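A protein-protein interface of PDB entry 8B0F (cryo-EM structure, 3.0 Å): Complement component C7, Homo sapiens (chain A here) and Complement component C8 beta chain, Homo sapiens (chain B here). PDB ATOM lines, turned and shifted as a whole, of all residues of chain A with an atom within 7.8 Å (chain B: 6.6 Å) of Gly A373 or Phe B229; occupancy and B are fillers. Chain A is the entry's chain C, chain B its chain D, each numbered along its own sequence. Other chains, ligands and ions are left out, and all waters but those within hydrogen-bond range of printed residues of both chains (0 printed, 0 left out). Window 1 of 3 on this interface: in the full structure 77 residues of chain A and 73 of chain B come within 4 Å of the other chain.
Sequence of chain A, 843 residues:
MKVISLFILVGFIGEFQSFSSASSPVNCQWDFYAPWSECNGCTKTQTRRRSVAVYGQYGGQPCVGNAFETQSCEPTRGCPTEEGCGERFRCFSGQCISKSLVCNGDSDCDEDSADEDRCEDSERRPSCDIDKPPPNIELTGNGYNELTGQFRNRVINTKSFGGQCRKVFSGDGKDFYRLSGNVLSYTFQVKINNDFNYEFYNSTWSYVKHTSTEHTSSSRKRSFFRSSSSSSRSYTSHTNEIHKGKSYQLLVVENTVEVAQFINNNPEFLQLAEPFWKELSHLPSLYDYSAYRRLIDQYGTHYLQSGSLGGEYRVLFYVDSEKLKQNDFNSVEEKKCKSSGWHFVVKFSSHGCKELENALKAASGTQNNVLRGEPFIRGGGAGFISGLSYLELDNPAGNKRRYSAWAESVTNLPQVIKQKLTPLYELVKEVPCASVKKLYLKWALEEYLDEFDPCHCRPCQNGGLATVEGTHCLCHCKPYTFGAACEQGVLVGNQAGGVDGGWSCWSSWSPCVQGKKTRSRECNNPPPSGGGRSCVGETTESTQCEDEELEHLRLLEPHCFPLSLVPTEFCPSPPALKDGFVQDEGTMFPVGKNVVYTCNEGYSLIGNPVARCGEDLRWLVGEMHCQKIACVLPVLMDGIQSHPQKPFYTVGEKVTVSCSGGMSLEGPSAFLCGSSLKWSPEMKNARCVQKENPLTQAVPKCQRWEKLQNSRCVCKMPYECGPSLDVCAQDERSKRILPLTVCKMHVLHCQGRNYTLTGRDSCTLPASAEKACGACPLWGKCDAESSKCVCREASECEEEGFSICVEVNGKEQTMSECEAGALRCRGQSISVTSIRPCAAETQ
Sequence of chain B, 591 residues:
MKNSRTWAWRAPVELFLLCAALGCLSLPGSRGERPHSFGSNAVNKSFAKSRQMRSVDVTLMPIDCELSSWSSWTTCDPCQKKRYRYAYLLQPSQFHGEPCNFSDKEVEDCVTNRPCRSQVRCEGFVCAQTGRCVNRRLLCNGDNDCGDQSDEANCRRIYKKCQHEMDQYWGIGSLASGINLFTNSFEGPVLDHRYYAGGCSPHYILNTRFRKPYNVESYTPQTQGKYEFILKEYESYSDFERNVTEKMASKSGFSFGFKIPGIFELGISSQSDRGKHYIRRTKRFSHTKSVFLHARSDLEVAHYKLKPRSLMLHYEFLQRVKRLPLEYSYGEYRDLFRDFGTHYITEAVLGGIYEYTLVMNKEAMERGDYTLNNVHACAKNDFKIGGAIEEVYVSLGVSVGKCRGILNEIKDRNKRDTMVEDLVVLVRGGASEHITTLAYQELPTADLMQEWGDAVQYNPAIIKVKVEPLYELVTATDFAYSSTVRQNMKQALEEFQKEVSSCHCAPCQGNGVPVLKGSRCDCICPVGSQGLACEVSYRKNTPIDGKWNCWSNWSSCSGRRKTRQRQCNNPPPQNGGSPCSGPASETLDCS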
ATOM      1  N   ARG A 314      -2.855   4.412  -8.482  1.00  0.00           N
ATOM      2  CA  ARG A 314      -3.452   5.694  -8.129  1.00  0.00           C
ATOM      3  C   ARG A 314      -4.303   5.545  -6.879  1.00  0.00           C
ATOM      4  O   ARG A 314      -5.075   4.590  -6.762  1.00  0.00           O
ATOM      5  CB  ARG A 314      -4.266   6.318  -9.270  1.00  0.00           C
ATOM      6  CG  ARG A 314      -3.487   6.496 -10.563  1.00  0.00           C
ATOM      7  CD  ARG A 314      -4.364   7.021 -11.691  1.00  0.00           C
ATOM      8  NE  ARG A 314      -5.140   6.007 -12.390  1.00  0.00           N
ATOM      9  CZ  ARG A 314      -4.642   5.198 -13.314  1.00  0.00           C
ATOM     10  NH1 ARG A 314      -3.398   5.324 -13.747  1.00  0.00           N
ATOM     11  NH2 ARG A 314      -5.421   4.262 -13.843  1.00  0.00           N
ATOM     12  N   VAL A 315      -4.156   6.484  -5.949  1.00  0.00           N
ATOM     13  CA  VAL A 315      -5.064   6.634  -4.819  1.00  0.00           C
ATOM     14  C   VAL A 315      -5.534   8.079  -4.776  1.00  0.00           C
ATOM     15  O   VAL A 315      -4.722   8.996  -4.616  1.00  0.00           O
ATOM     16  CB  VAL A 315      -4.393   6.258  -3.489  1.00  0.00           C
ATOM     17  CG1 VAL A 315      -5.403   6.283  -2.359  1.00  0.00           C
ATOM     18  CG2 VAL A 315      -3.732   4.905  -3.591  1.00  0.00           C
ATOM     19  N   LEU A 316      -6.841   8.280  -4.936  1.00  0.00           N
ATOM     20  CA  LEU A 316      -7.528   9.477  -4.468  1.00  0.00           C
ATOM     21  C   LEU A 316      -8.257   9.137  -3.174  1.00  0.00           C
ATOM     22  O   LEU A 316      -9.101   8.237  -3.154  1.00  0.00           O
ATOM     23  CB  LEU A 316      -8.506   9.986  -5.524  1.00  0.00           C
ATOM     24  CG  LEU A 316      -9.392  11.160  -5.120  1.00  0.00           C
ATOM     25  CD1 LEU A 316      -8.551  12.398  -4.919  1.00  0.00           C
ATOM     26  CD2 LEU A 316     -10.455  11.407  -6.165  1.00  0.00           C
ATOM     27  N   PHE A 317      -7.931   9.855  -2.103  1.00  0.00           N
ATOM     28  CA  PHE A 317      -8.556   9.678  -0.799  1.00  0.00           C
ATOM     29  C   PHE A 317      -8.986  11.032  -0.255  1.00  0.00           C
ATOM     30  O   PHE A 317      -8.184  11.966  -0.220  1.00  0.00           O
ATOM     31  CB  PHE A 317      -7.567   8.978   0.136  1.00  0.00           C
ATOM     32  CG  PHE A 317      -8.018   8.878   1.556  1.00  0.00           C
ATOM     33  CD1 PHE A 317      -8.934   7.917   1.933  1.00  0.00           C
ATOM     34  CD2 PHE A 317      -7.535   9.748   2.511  1.00  0.00           C
ATOM     35  CE1 PHE A 317      -9.358   7.826   3.235  1.00  0.00           C
ATOM     36  CE2 PHE A 317      -7.957   9.659   3.816  1.00  0.00           C
ATOM     37  CZ  PHE A 317      -8.864   8.691   4.179  1.00  0.00           C
ATOM     38  N   TYR A 318     -10.249  11.142   0.166  1.00  0.00           N
ATOM     39  CA  TYR A 318     -10.828  12.409   0.602  1.00  0.00           C
ATOM     40  C   TYR A 318     -11.566  12.215   1.920  1.00  0.00           C
ATOM     41  O   TYR A 318     -12.462  11.374   2.013  1.00  0.00           O
ATOM     42  CB  TYR A 318     -11.766  12.916  -0.498  1.00  0.00           C
ATOM     43  CG  TYR A 318     -12.576  14.153  -0.215  1.00  0.00           C
ATOM     44  CD1 TYR A 318     -12.005  15.413  -0.271  1.00  0.00           C
ATOM     45  CD2 TYR A 318     -13.927  14.061   0.077  1.00  0.00           C
ATOM     46  CE1 TYR A 318     -12.748  16.540  -0.010  1.00  0.00           C
ATOM     47  CE2 TYR A 318     -14.679  15.181   0.329  1.00  0.00           C
ATOM     48  CZ  TYR A 318     -14.088  16.418   0.272  1.00  0.00           C
ATOM     49  OH  TYR A 318     -14.845  17.542   0.499  1.00  0.00           O
ATOM     50  N   VAL A 319     -11.178  12.991   2.933  1.00  0.00           N
ATOM     51  CA  VAL A 319     -11.850  13.085   4.231  1.00  0.00           C
ATOM     52  C   VAL A 319     -12.398  14.495   4.422  1.00  0.00           C
ATOM     53  O   VAL A 319     -11.638  15.468   4.374  1.00  0.00           O
ATOM     54  CB  VAL A 319     -10.913  12.705   5.386  1.00  0.00           C
ATOM     55  CG1 VAL A 319     -11.661  12.722   6.705  1.00  0.00           C
ATOM     56  CG2 VAL A 319     -10.325  11.335   5.155  1.00  0.00           C
ATOM     57  N   LEU A 371     -16.048  10.262   4.081  1.00  0.00           N
ATOM     58  CA  LEU A 371     -14.741   9.736   3.710  1.00  0.00           C
ATOM     59  C   LEU A 371     -14.895   8.917   2.438  1.00  0.00           C
ATOM     60  O   LEU A 371     -15.782   8.065   2.351  1.00  0.00           O
ATOM     61  CB  LEU A 371     -14.166   8.889   4.850  1.00  0.00           C
ATOM     62  CG  LEU A 371     -12.788   8.248   4.695  1.00  0.00           C
ATOM     63  CD1 LEU A 371     -12.304   7.761   6.046  1.00  0.00           C
ATOM     64  CD2 LEU A 371     -12.812   7.097   3.710  1.00  0.00           C
ATOM     65  N   ARG A 372     -14.037   9.180   1.453  1.00  0.00           N
ATOM     66  CA  ARG A 372     -14.088   8.504   0.164  1.00  0.00           C
ATOM     67  C   ARG A 372     -12.682   8.148  -0.291  1.00  0.00           C
ATOM     68  O   ARG A 372     -11.751   8.935  -0.104  1.00  0.00           O
ATOM     69  CB  ARG A 372     -14.760   9.388  -0.889  1.00  0.00           C
ATOM     70  CG  ARG A 372     -16.120   9.916  -0.482  1.00  0.00           C
ATOM     71  CD  ARG A 372     -16.812  10.598  -1.642  1.00  0.00           C
ATOM     72  NE  ARG A 372     -18.002  11.328  -1.225  1.00  0.00           N
ATOM     73  CZ  ARG A 372     -19.166  11.323  -1.860  1.00  0.00           C
ATOM     74  NH1 ARG A 372     -19.447  10.430  -2.794  1.00  0.00           N
ATOM     75  NH2 ARG A 372     -20.067  12.256  -1.565  1.00  0.00           N
ATOM     76  N   GLY A 373     -12.528   6.972  -0.892  1.00  0.00           N
ATOM     77  CA  GLY A 373     -11.227   6.550  -1.379  1.00  0.00           C
ATOM     78  C   GLY A 373     -11.299   5.534  -2.502  1.00  0.00           C
ATOM     79  O   GLY A 373     -12.127   4.623  -2.462  1.00  0.00           O
ATOM     80  N   GLU A 374     -10.446   5.685  -3.515  1.00  0.00           N
ATOM     81  CA  GLU A 374     -10.479   4.838  -4.709  1.00  0.00           C
ATOM     82  C   GLU A 374      -9.071   4.447  -5.133  1.00  0.00           C
ATOM     83  O   GLU A 374      -8.530   4.976  -6.111  1.00  0.00           O
ATOM     84  CB  GLU A 374     -11.191   5.546  -5.862  1.00  0.00           C
ATOM     85  CG  GLU A 374     -12.643   5.873  -5.599  1.00  0.00           C
ATOM     86  CD  GLU A 374     -13.180   6.916  -6.559  1.00  0.00           C
ATOM     87  OE1 GLU A 374     -12.911   8.117  -6.345  1.00  0.00           O
ATOM     88  OE2 GLU A 374     -13.867   6.533  -7.530  1.00  0.00           O
ATOM     89  N   PRO A 375      -8.441   3.518  -4.419  1.00  0.00           N
ATOM     90  CA  PRO A 375      -7.201   2.918  -4.926  1.00  0.00           C
ATOM     91  C   PRO A 375      -7.447   2.145  -6.213  1.00  0.00           C
ATOM     92  O   PRO A 375      -8.363   1.326  -6.296  1.00  0.00           O
ATOM     93  CB  PRO A 375      -6.764   1.995  -3.782  1.00  0.00           C
ATOM     94  CG  PRO A 375      -7.423   2.564  -2.579  1.00  0.00           C
ATOM     95  CD  PRO A 375      -8.759   3.017  -3.078  1.00  0.00           C
ATOM     96  N   PHE A 376      -6.628   2.414  -7.225  1.00  0.00           N
ATOM     97  CA  PHE A 376      -6.725   1.722  -8.502  1.00  0.00           C
ATOM     98  C   PHE A 376      -5.349   1.232  -8.929  1.00  0.00           C
ATOM     99  O   PHE A 376      -4.364   1.967  -8.827  1.00  0.00           O
ATOM    100  CB  PHE A 376      -7.309   2.637  -9.575  1.00  0.00           C
ATOM    101  CG  PHE A 376      -7.384   2.008 -10.930  1.00  0.00           C
ATOM    102  CD1 PHE A 376      -8.485   1.259 -11.295  1.00  0.00           C
ATOM    103  CD2 PHE A 376      -6.357   2.160 -11.837  1.00  0.00           C
ATOM    104  CE1 PHE A 376      -8.558   0.678 -12.538  1.00  0.00           C
ATOM    105  CE2 PHE A 376      -6.424   1.568 -13.078  1.00  0.00           C
ATOM    106  CZ  PHE A 376      -7.525   0.829 -13.427  1.00  0.00           C
ATOM    107  N   SER A 389      -4.613  -2.451  -3.001  1.00  0.00           N
ATOM    108  CA  SER A 389      -5.759  -1.596  -3.290  1.00  0.00           C
ATOM    109  C   SER A 389      -6.794  -1.567  -2.174  1.00  0.00           C
ATOM    110  O   SER A 389      -7.648  -0.678  -2.175  1.00  0.00           O
ATOM    111  CB  SER A 389      -6.433  -2.041  -4.586  1.00  0.00           C
ATOM    112  OG  SER A 389      -6.933  -3.358  -4.470  1.00  0.00           O
ATOM    113  N   TYR A 390      -6.752  -2.498  -1.226  1.00  0.00           N
ATOM    114  CA  TYR A 390      -7.630  -2.402  -0.064  1.00  0.00           C
ATOM    115  C   TYR A 390      -7.215  -1.218   0.799  1.00  0.00           C
ATOM    116  O   TYR A 390      -6.139  -1.221   1.403  1.00  0.00           O
ATOM    117  CB  TYR A 390      -7.599  -3.696   0.737  1.00  0.00           C
ATOM    118  CG  TYR A 390      -8.531  -3.678   1.922  1.00  0.00           C
ATOM    119  CD1 TYR A 390      -9.901  -3.779   1.747  1.00  0.00           C
ATOM    120  CD2 TYR A 390      -8.045  -3.539   3.211  1.00  0.00           C
ATOM    121  CE1 TYR A 390     -10.759  -3.744   2.818  1.00  0.00           C
ATOM    122  CE2 TYR A 390      -8.897  -3.503   4.289  1.00  0.00           C
ATOM    123  CZ  TYR A 390     -10.253  -3.610   4.087  1.00  0.00           C
ATOM    124  OH  TYR A 390     -11.105  -3.590   5.163  1.00  0.00           O
ATOM    125  N   LEU A 391      -8.078  -0.207   0.858  1.00  0.00           N
ATOM    126  CA  LEU A 391      -7.763   1.052   1.523  1.00  0.00           C
ATOM    127  C   LEU A 391      -7.654   0.858   3.031  1.00  0.00           C
ATOM    128  O   LEU A 391      -8.637   0.504   3.690  1.00  0.00           O
ATOM    129  CB  LEU A 391      -8.838   2.084   1.196  1.00  0.00           C
ATOM    130  CG  LEU A 391      -8.575   3.529   1.609  1.00  0.00           C
ATOM    131  CD1 LEU A 391      -7.632   4.201   0.631  1.00  0.00           C
ATOM    132  CD2 LEU A 391      -9.882   4.288   1.701  1.00  0.00           C
ATOM    133  N   GLU A 392      -6.463   1.090   3.576  1.00  0.00           N
ATOM    134  CA  GLU A 392      -6.241   1.094   5.019  1.00  0.00           C
ATOM    135  C   GLU A 392      -6.377   2.527   5.520  1.00  0.00           C
ATOM    136  O   GLU A 392      -5.531   3.375   5.219  1.00  0.00           O
ATOM    137  CB  GLU A 392      -4.868   0.522   5.357  1.00  0.00           C
ATOM    138  CG  GLU A 392      -4.693  -0.930   4.957  1.00  0.00           C
ATOM    139  CD  GLU A 392      -3.400  -1.525   5.473  1.00  0.00           C
ATOM    140  OE1 GLU A 392      -2.321  -1.093   5.016  1.00  0.00           O
ATOM    141  OE2 GLU A 392      -3.461  -2.425   6.336  1.00  0.00           O
ATOM    142  N   LEU A 393      -7.432   2.803   6.288  1.00  0.00           N
ATOM    143  CA  LEU A 393      -7.783   4.189   6.570  1.00  0.00           C
ATOM    144  C   LEU A 393      -6.732   4.907   7.404  1.00  0.00           C
ATOM    145  O   LEU A 393      -6.674   6.140   7.372  1.00  0.00           O
ATOM    146  CB  LEU A 393      -9.125   4.254   7.301  1.00  0.00           C
ATOM    147  CG  LEU A 393     -10.334   3.623   6.612  1.00  0.00           C
ATOM    148  CD1 LEU A 393     -11.598   3.949   7.383  1.00  0.00           C
ATOM    149  CD2 LEU A 393     -10.453   4.095   5.176  1.00  0.00           C
ATOM    150  N   PRO A 396      -3.530   5.578   4.045  1.00  0.00           N
ATOM    151  CA  PRO A 396      -4.319   5.406   2.818  1.00  0.00           C
ATOM    152  C   PRO A 396      -3.476   5.281   1.562  1.00  0.00           C
ATOM    153  O   PRO A 396      -3.964   4.732   0.568  1.00  0.00           O
ATOM    154  CB  PRO A 396      -5.188   6.672   2.777  1.00  0.00           C
ATOM    155  CG  PRO A 396      -5.155   7.217   4.158  1.00  0.00           C
ATOM    156  CD  PRO A 396      -3.803   6.871   4.683  1.00  0.00           C
ATOM    157  N   TYR A 480     -16.339  12.565  -7.323  1.00  0.00           N
ATOM    158  CA  TYR A 480     -17.372  13.010  -6.392  1.00  0.00           C
ATOM    159  C   TYR A 480     -18.361  13.975  -7.034  1.00  0.00           C
ATOM    160  O   TYR A 480     -18.987  14.787  -6.353  1.00  0.00           O
ATOM    161  CB  TYR A 480     -16.726  13.614  -5.147  1.00  0.00           C
ATOM    162  CG  TYR A 480     -15.554  12.785  -4.676  1.00  0.00           C
ATOM    163  CD1 TYR A 480     -15.599  11.401  -4.718  1.00  0.00           C
ATOM    164  CD2 TYR A 480     -14.418  13.380  -4.158  1.00  0.00           C
ATOM    165  CE1 TYR A 480     -14.555  10.640  -4.255  1.00  0.00           C
ATOM    166  CE2 TYR A 480     -13.355  12.624  -3.714  1.00  0.00           C
ATOM    167  CZ  TYR A 480     -13.428  11.255  -3.769  1.00  0.00           C
ATOM    168  OH  TYR A 480     -12.359  10.493  -3.366  1.00  0.00           O
ATOM    169  N   TYR B 227     -10.542  -0.700  -5.948  1.00  0.00           N
ATOM    170  CA  TYR B 227     -11.267  -0.676  -4.683  1.00  0.00           C
ATOM    171  C   TYR B 227     -11.928   0.682  -4.490  1.00  0.00           C
ATOM    172  O   TYR B 227     -11.270   1.717  -4.614  1.00  0.00           O
ATOM    173  CB  TYR B 227     -10.320  -0.966  -3.520  1.00  0.00           C
ATOM    174  CG  TYR B 227     -10.995  -1.083  -2.178  1.00  0.00           C
ATOM    175  CD1 TYR B 227     -11.779  -2.181  -1.869  1.00  0.00           C
ATOM    176  CD2 TYR B 227     -10.836  -0.103  -1.213  1.00  0.00           C
ATOM    177  CE1 TYR B 227     -12.394  -2.294  -0.647  1.00  0.00           C
ATOM    178  CE2 TYR B 227     -11.447  -0.211   0.015  1.00  0.00           C
ATOM    179  CZ  TYR B 227     -12.230  -1.305   0.289  1.00  0.00           C
ATOM    180  OH  TYR B 227     -12.837  -1.420   1.515  1.00  0.00           O
ATOM    181  N   GLU B 228     -13.226   0.673  -4.191  1.00  0.00           N
ATOM    182  CA  GLU B 228     -13.993   1.876  -3.886  1.00  0.00           C
ATOM    183  C   GLU B 228     -14.493   1.804  -2.450  1.00  0.00           C
ATOM    184  O   GLU B 228     -15.206   0.864  -2.089  1.00  0.00           O
ATOM    185  CB  GLU B 228     -15.158   2.033  -4.861  1.00  0.00           C
ATOM    186  CG  GLU B 228     -16.123   3.153  -4.524  1.00  0.00           C
ATOM    187  CD  GLU B 228     -17.383   3.097  -5.356  1.00  0.00           C
ATOM    188  OE1 GLU B 228     -18.115   2.090  -5.258  1.00  0.00           O
ATOM    189  OE2 GLU B 228     -17.644   4.060  -6.109  1.00  0.00           O
ATOM    190  N   PHE B 229     -14.131   2.797  -1.641  1.00  0.00           N
ATOM    191  CA  PHE B 229     -14.607   2.917  -0.268  1.00  0.00           C
ATOM    192  C   PHE B 229     -15.368   4.223  -0.093  1.00  0.00           C
ATOM    193  O   PHE B 229     -14.904   5.278  -0.531  1.00  0.00           O
ATOM    194  CB  PHE B 229     -13.435   2.862   0.711  1.00  0.00           C
ATOM    195  CG  PHE B 229     -13.847   2.796   2.148  1.00  0.00           C
ATOM    196  CD1 PHE B 229     -14.128   1.583   2.748  1.00  0.00           C
ATOM    197  CD2 PHE B 229     -13.953   3.946   2.902  1.00  0.00           C
ATOM    198  CE1 PHE B 229     -14.508   1.524   4.068  1.00  0.00           C
ATOM    199  CE2 PHE B 229     -14.332   3.890   4.224  1.00  0.00           C
ATOM    200  CZ  PHE B 229     -14.606   2.678   4.808  1.00  0.00           C
ATOM    201  N   ILE B 230     -16.536   4.148   0.541  1.00  0.00           N
ATOM    202  CA  ILE B 230     -17.349   5.321   0.848  1.00  0.00           C
ATOM    203  C   ILE B 230     -17.911   5.156   2.252  1.00  0.00           C
ATOM    204  O   ILE B 230     -18.479   4.111   2.576  1.00  0.00           O
ATOM    205  CB  ILE B 230     -18.494   5.509  -0.166  1.00  0.00           C
ATOM    206  CG1 ILE B 230     -17.933   5.650  -1.579  1.00  0.00           C
ATOM    207  CG2 ILE B 230     -19.325   6.728   0.194  1.00  0.00           C
ATOM    208  CD1 ILE B 230     -18.987   5.617  -2.657  1.00  0.00           C
ATOM    209  N   LEU B 231     -17.758   6.185   3.082  1.00  0.00           N
ATOM    210  CA  LEU B 231     -18.284   6.178   4.446  1.00  0.00           C
ATOM    211  C   LEU B 231     -18.852   7.556   4.746  1.00  0.00           C
ATOM    212  O   LEU B 231     -18.094   8.516   4.900  1.00  0.00           O
ATOM    213  CB  LEU B 231     -17.201   5.801   5.455  1.00  0.00           C
ATOM    214  CG  LEU B 231     -17.542   6.029   6.924  1.00  0.00           C
ATOM    215  CD1 LEU B 231     -18.750   5.209   7.323  1.00  0.00           C
ATOM    216  CD2 LEU B 231     -16.354   5.677   7.792  1.00  0.00           C
ATOM    217  N   LEU B 293     -22.120   3.015   4.699  1.00  0.00           N
ATOM    218  CA  LEU B 293     -20.765   2.498   4.510  1.00  0.00           C
ATOM    219  C   LEU B 293     -20.799   1.476   3.381  1.00  0.00           C
ATOM    220  O   LEU B 293     -21.252   0.346   3.575  1.00  0.00           O
ATOM    221  CB  LEU B 293     -20.237   1.883   5.800  1.00  0.00           C
ATOM    222  CG  LEU B 293     -18.995   1.002   5.696  1.00  0.00           C
ATOM    223  CD1 LEU B 293     -17.881   1.694   4.941  1.00  0.00           C
ATOM    224  CD2 LEU B 293     -18.529   0.615   7.083  1.00  0.00           C
ATOM    225  N   HIS B 294     -20.324   1.873   2.205  1.00  0.00           N
ATOM    226  CA  HIS B 294     -20.249   0.999   1.043  1.00  0.00           C
ATOM    227  C   HIS B 294     -18.791   0.781   0.676  1.00  0.00           C
ATOM    228  O   HIS B 294     -18.037   1.745   0.521  1.00  0.00           O
ATOM    229  CB  HIS B 294     -21.021   1.605  -0.131  1.00  0.00           C
ATOM    230  CG  HIS B 294     -20.733   0.960  -1.449  1.00  0.00           C
ATOM    231  ND1 HIS B 294     -21.535  -0.025  -1.983  1.00  0.00           N
ATOM    232  CD2 HIS B 294     -19.709   1.123  -2.318  1.00  0.00           C
ATOM    233  CE1 HIS B 294     -21.042  -0.405  -3.148  1.00  0.00           C
ATOM    234  NE2 HIS B 294     -19.926   0.265  -3.367  1.00  0.00           N
ATOM    235  N   ALA B 295     -18.397  -0.483   0.547  1.00  0.00           N
ATOM    236  CA  ALA B 295     -17.088  -0.869   0.043  1.00  0.00           C
ATOM    237  C   ALA B 295     -17.257  -1.847  -1.107  1.00  0.00           C
ATOM    238  O   ALA B 295     -18.117  -2.728  -1.057  1.00  0.00           O
ATOM    239  CB  ALA B 295     -16.234  -1.503   1.140  1.00  0.00           C
ATOM    240  N   ARG B 296     -16.443  -1.688  -2.147  1.00  0.00           N
ATOM    241  CA  ARG B 296     -16.457  -2.620  -3.269  1.00  0.00           C
ATOM    242  C   ARG B 296     -15.048  -2.780  -3.809  1.00  0.00           C
ATOM    243  O   ARG B 296     -14.423  -1.798  -4.214  1.00  0.00           O
ATOM    244  CB  ARG B 296     -17.390  -2.136  -4.379  1.00  0.00           C
ATOM    245  CG  ARG B 296     -17.419  -3.063  -5.577  1.00  0.00           C
ATOM    246  CD  ARG B 296     -18.357  -2.575  -6.654  1.00  0.00           C
ATOM    247  NE  ARG B 296     -19.455  -3.505  -6.875  1.00  0.00           N
ATOM    248  CZ  ARG B 296     -19.591  -4.275  -7.947  1.00  0.00           C
ATOM    249  NH1 ARG B 296     -18.633  -4.378  -8.854  1.00  0.00           N
ATOM    250  NH2 ARG B 296     -20.706  -4.983  -8.101  1.00  0.00           N
ATOM    251  N   LEU B 443     -15.669  -5.636   7.993  1.00  0.00           N
ATOM    252  CA  LEU B 443     -14.727  -5.402   6.911  1.00  0.00           C
ATOM    253  C   LEU B 443     -13.446  -6.208   7.129  1.00  0.00           C
ATOM    254  O   LEU B 443     -13.017  -6.413   8.267  1.00  0.00           O
ATOM    255  CB  LEU B 443     -14.393  -3.917   6.814  1.00  0.00           C
ATOM    256  CG  LEU B 443     -15.464  -3.016   6.203  1.00  0.00           C
ATOM    257  CD1 LEU B 443     -15.134  -1.563   6.467  1.00  0.00           C
ATOM    258  CD2 LEU B 443     -15.590  -3.265   4.714  1.00  0.00           C
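The backbone NH (N) of Leu A371 is in hydrogen-bond range of the backbone carbonyl oxygen (O) of Leu B231 (2.8 Å).
The backbone carbonyl oxygen of Gly A373 is in hydrogen-bond range of the backbone NH of Phe B229 (2.8 Å).
O of Pro A375 sits at hydrogen-bond distance from N of Tyr B227, 3.0 Å away.
N of Glu A374 sits at hydrogen-bond distance from O of Leu A316, 2.9 Å away.
The backbone carbonyl oxygen (O) of Arg A372 sits at hydrogen-bond distance from the backbone NH (N) of Tyr A318, at 2.7 Å.
NE2 of His B294 is in hydrogen-bond range of OE1 of Glu B228 (3.2 Å).
O of Arg B296 sits at hydrogen-bond distance from N of Glu B228 (2.7 Å).
O of His B294 lies within hydrogen-bond range of N of Ile B230 (2.8 Å).
Leu A371 touches Phe B229.
CA of Arg A372 touches O of Phe B229, at 3.4 Å.
O of Gly A373 touches O of Tyr B227, 3.7 Å away.
O of Gly A373 touches CA of Glu B228, 3.6 Å away.
O of Tyr B227 touches CA of Glu A374 (3.2 Å).
CB of Tyr B227 touches O of Ser A389, at 3.0 Å.
Leu B443 touches Tyr A390.
CD2 of Tyr B227 touches N of Leu A391, 3.5 Å away.
CB of Phe B229 touches CD2 of Leu A391, 3.95 Å away.
Leu A393 touches Phe B229.
Of the printed residues of chain B, Leu A371 touches Phe B229, Ile B230 and Leu B231.
Of the printed residues of chain B, Tyr A390 touches Tyr B227 and Leu B443.
Glu A392 touches none of the printed residues of chain B.
Of the printed residues of chain A, Glu B228 touches Gly A373 (3.6 Å).
Of the printed residues of chain A, Phe B229 touches Leu A371 (3.4 Å), Arg A372 (3.4 Å), Gly A373 (2.8 Å), Leu A391 (3.95 Å) and Leu A393 (3.999 Å).
Of the printed residues of chain A, Leu B231 touches Leu A371.
The nearest residue of chain B that does not touch Gly A373 is Ile B230 (5.1 Å).
The nearest printed residue of chain B that does not touch Ser A389 is Glu B228 (6.1 Å).
Hydrophobic or aromatic side chains of chain A that line the printed part of chain B: Leu A371, Pro A375, Tyr A390, Leu A391 and Leu A393.
Of the 10 printed residues of chain B, 6 touch a printed residue of chain A.
Among the printed residues, no Asp or Glu carboxylate lies within 4 Å of a Lys or Arg side-chain nitrogen of the other chain.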
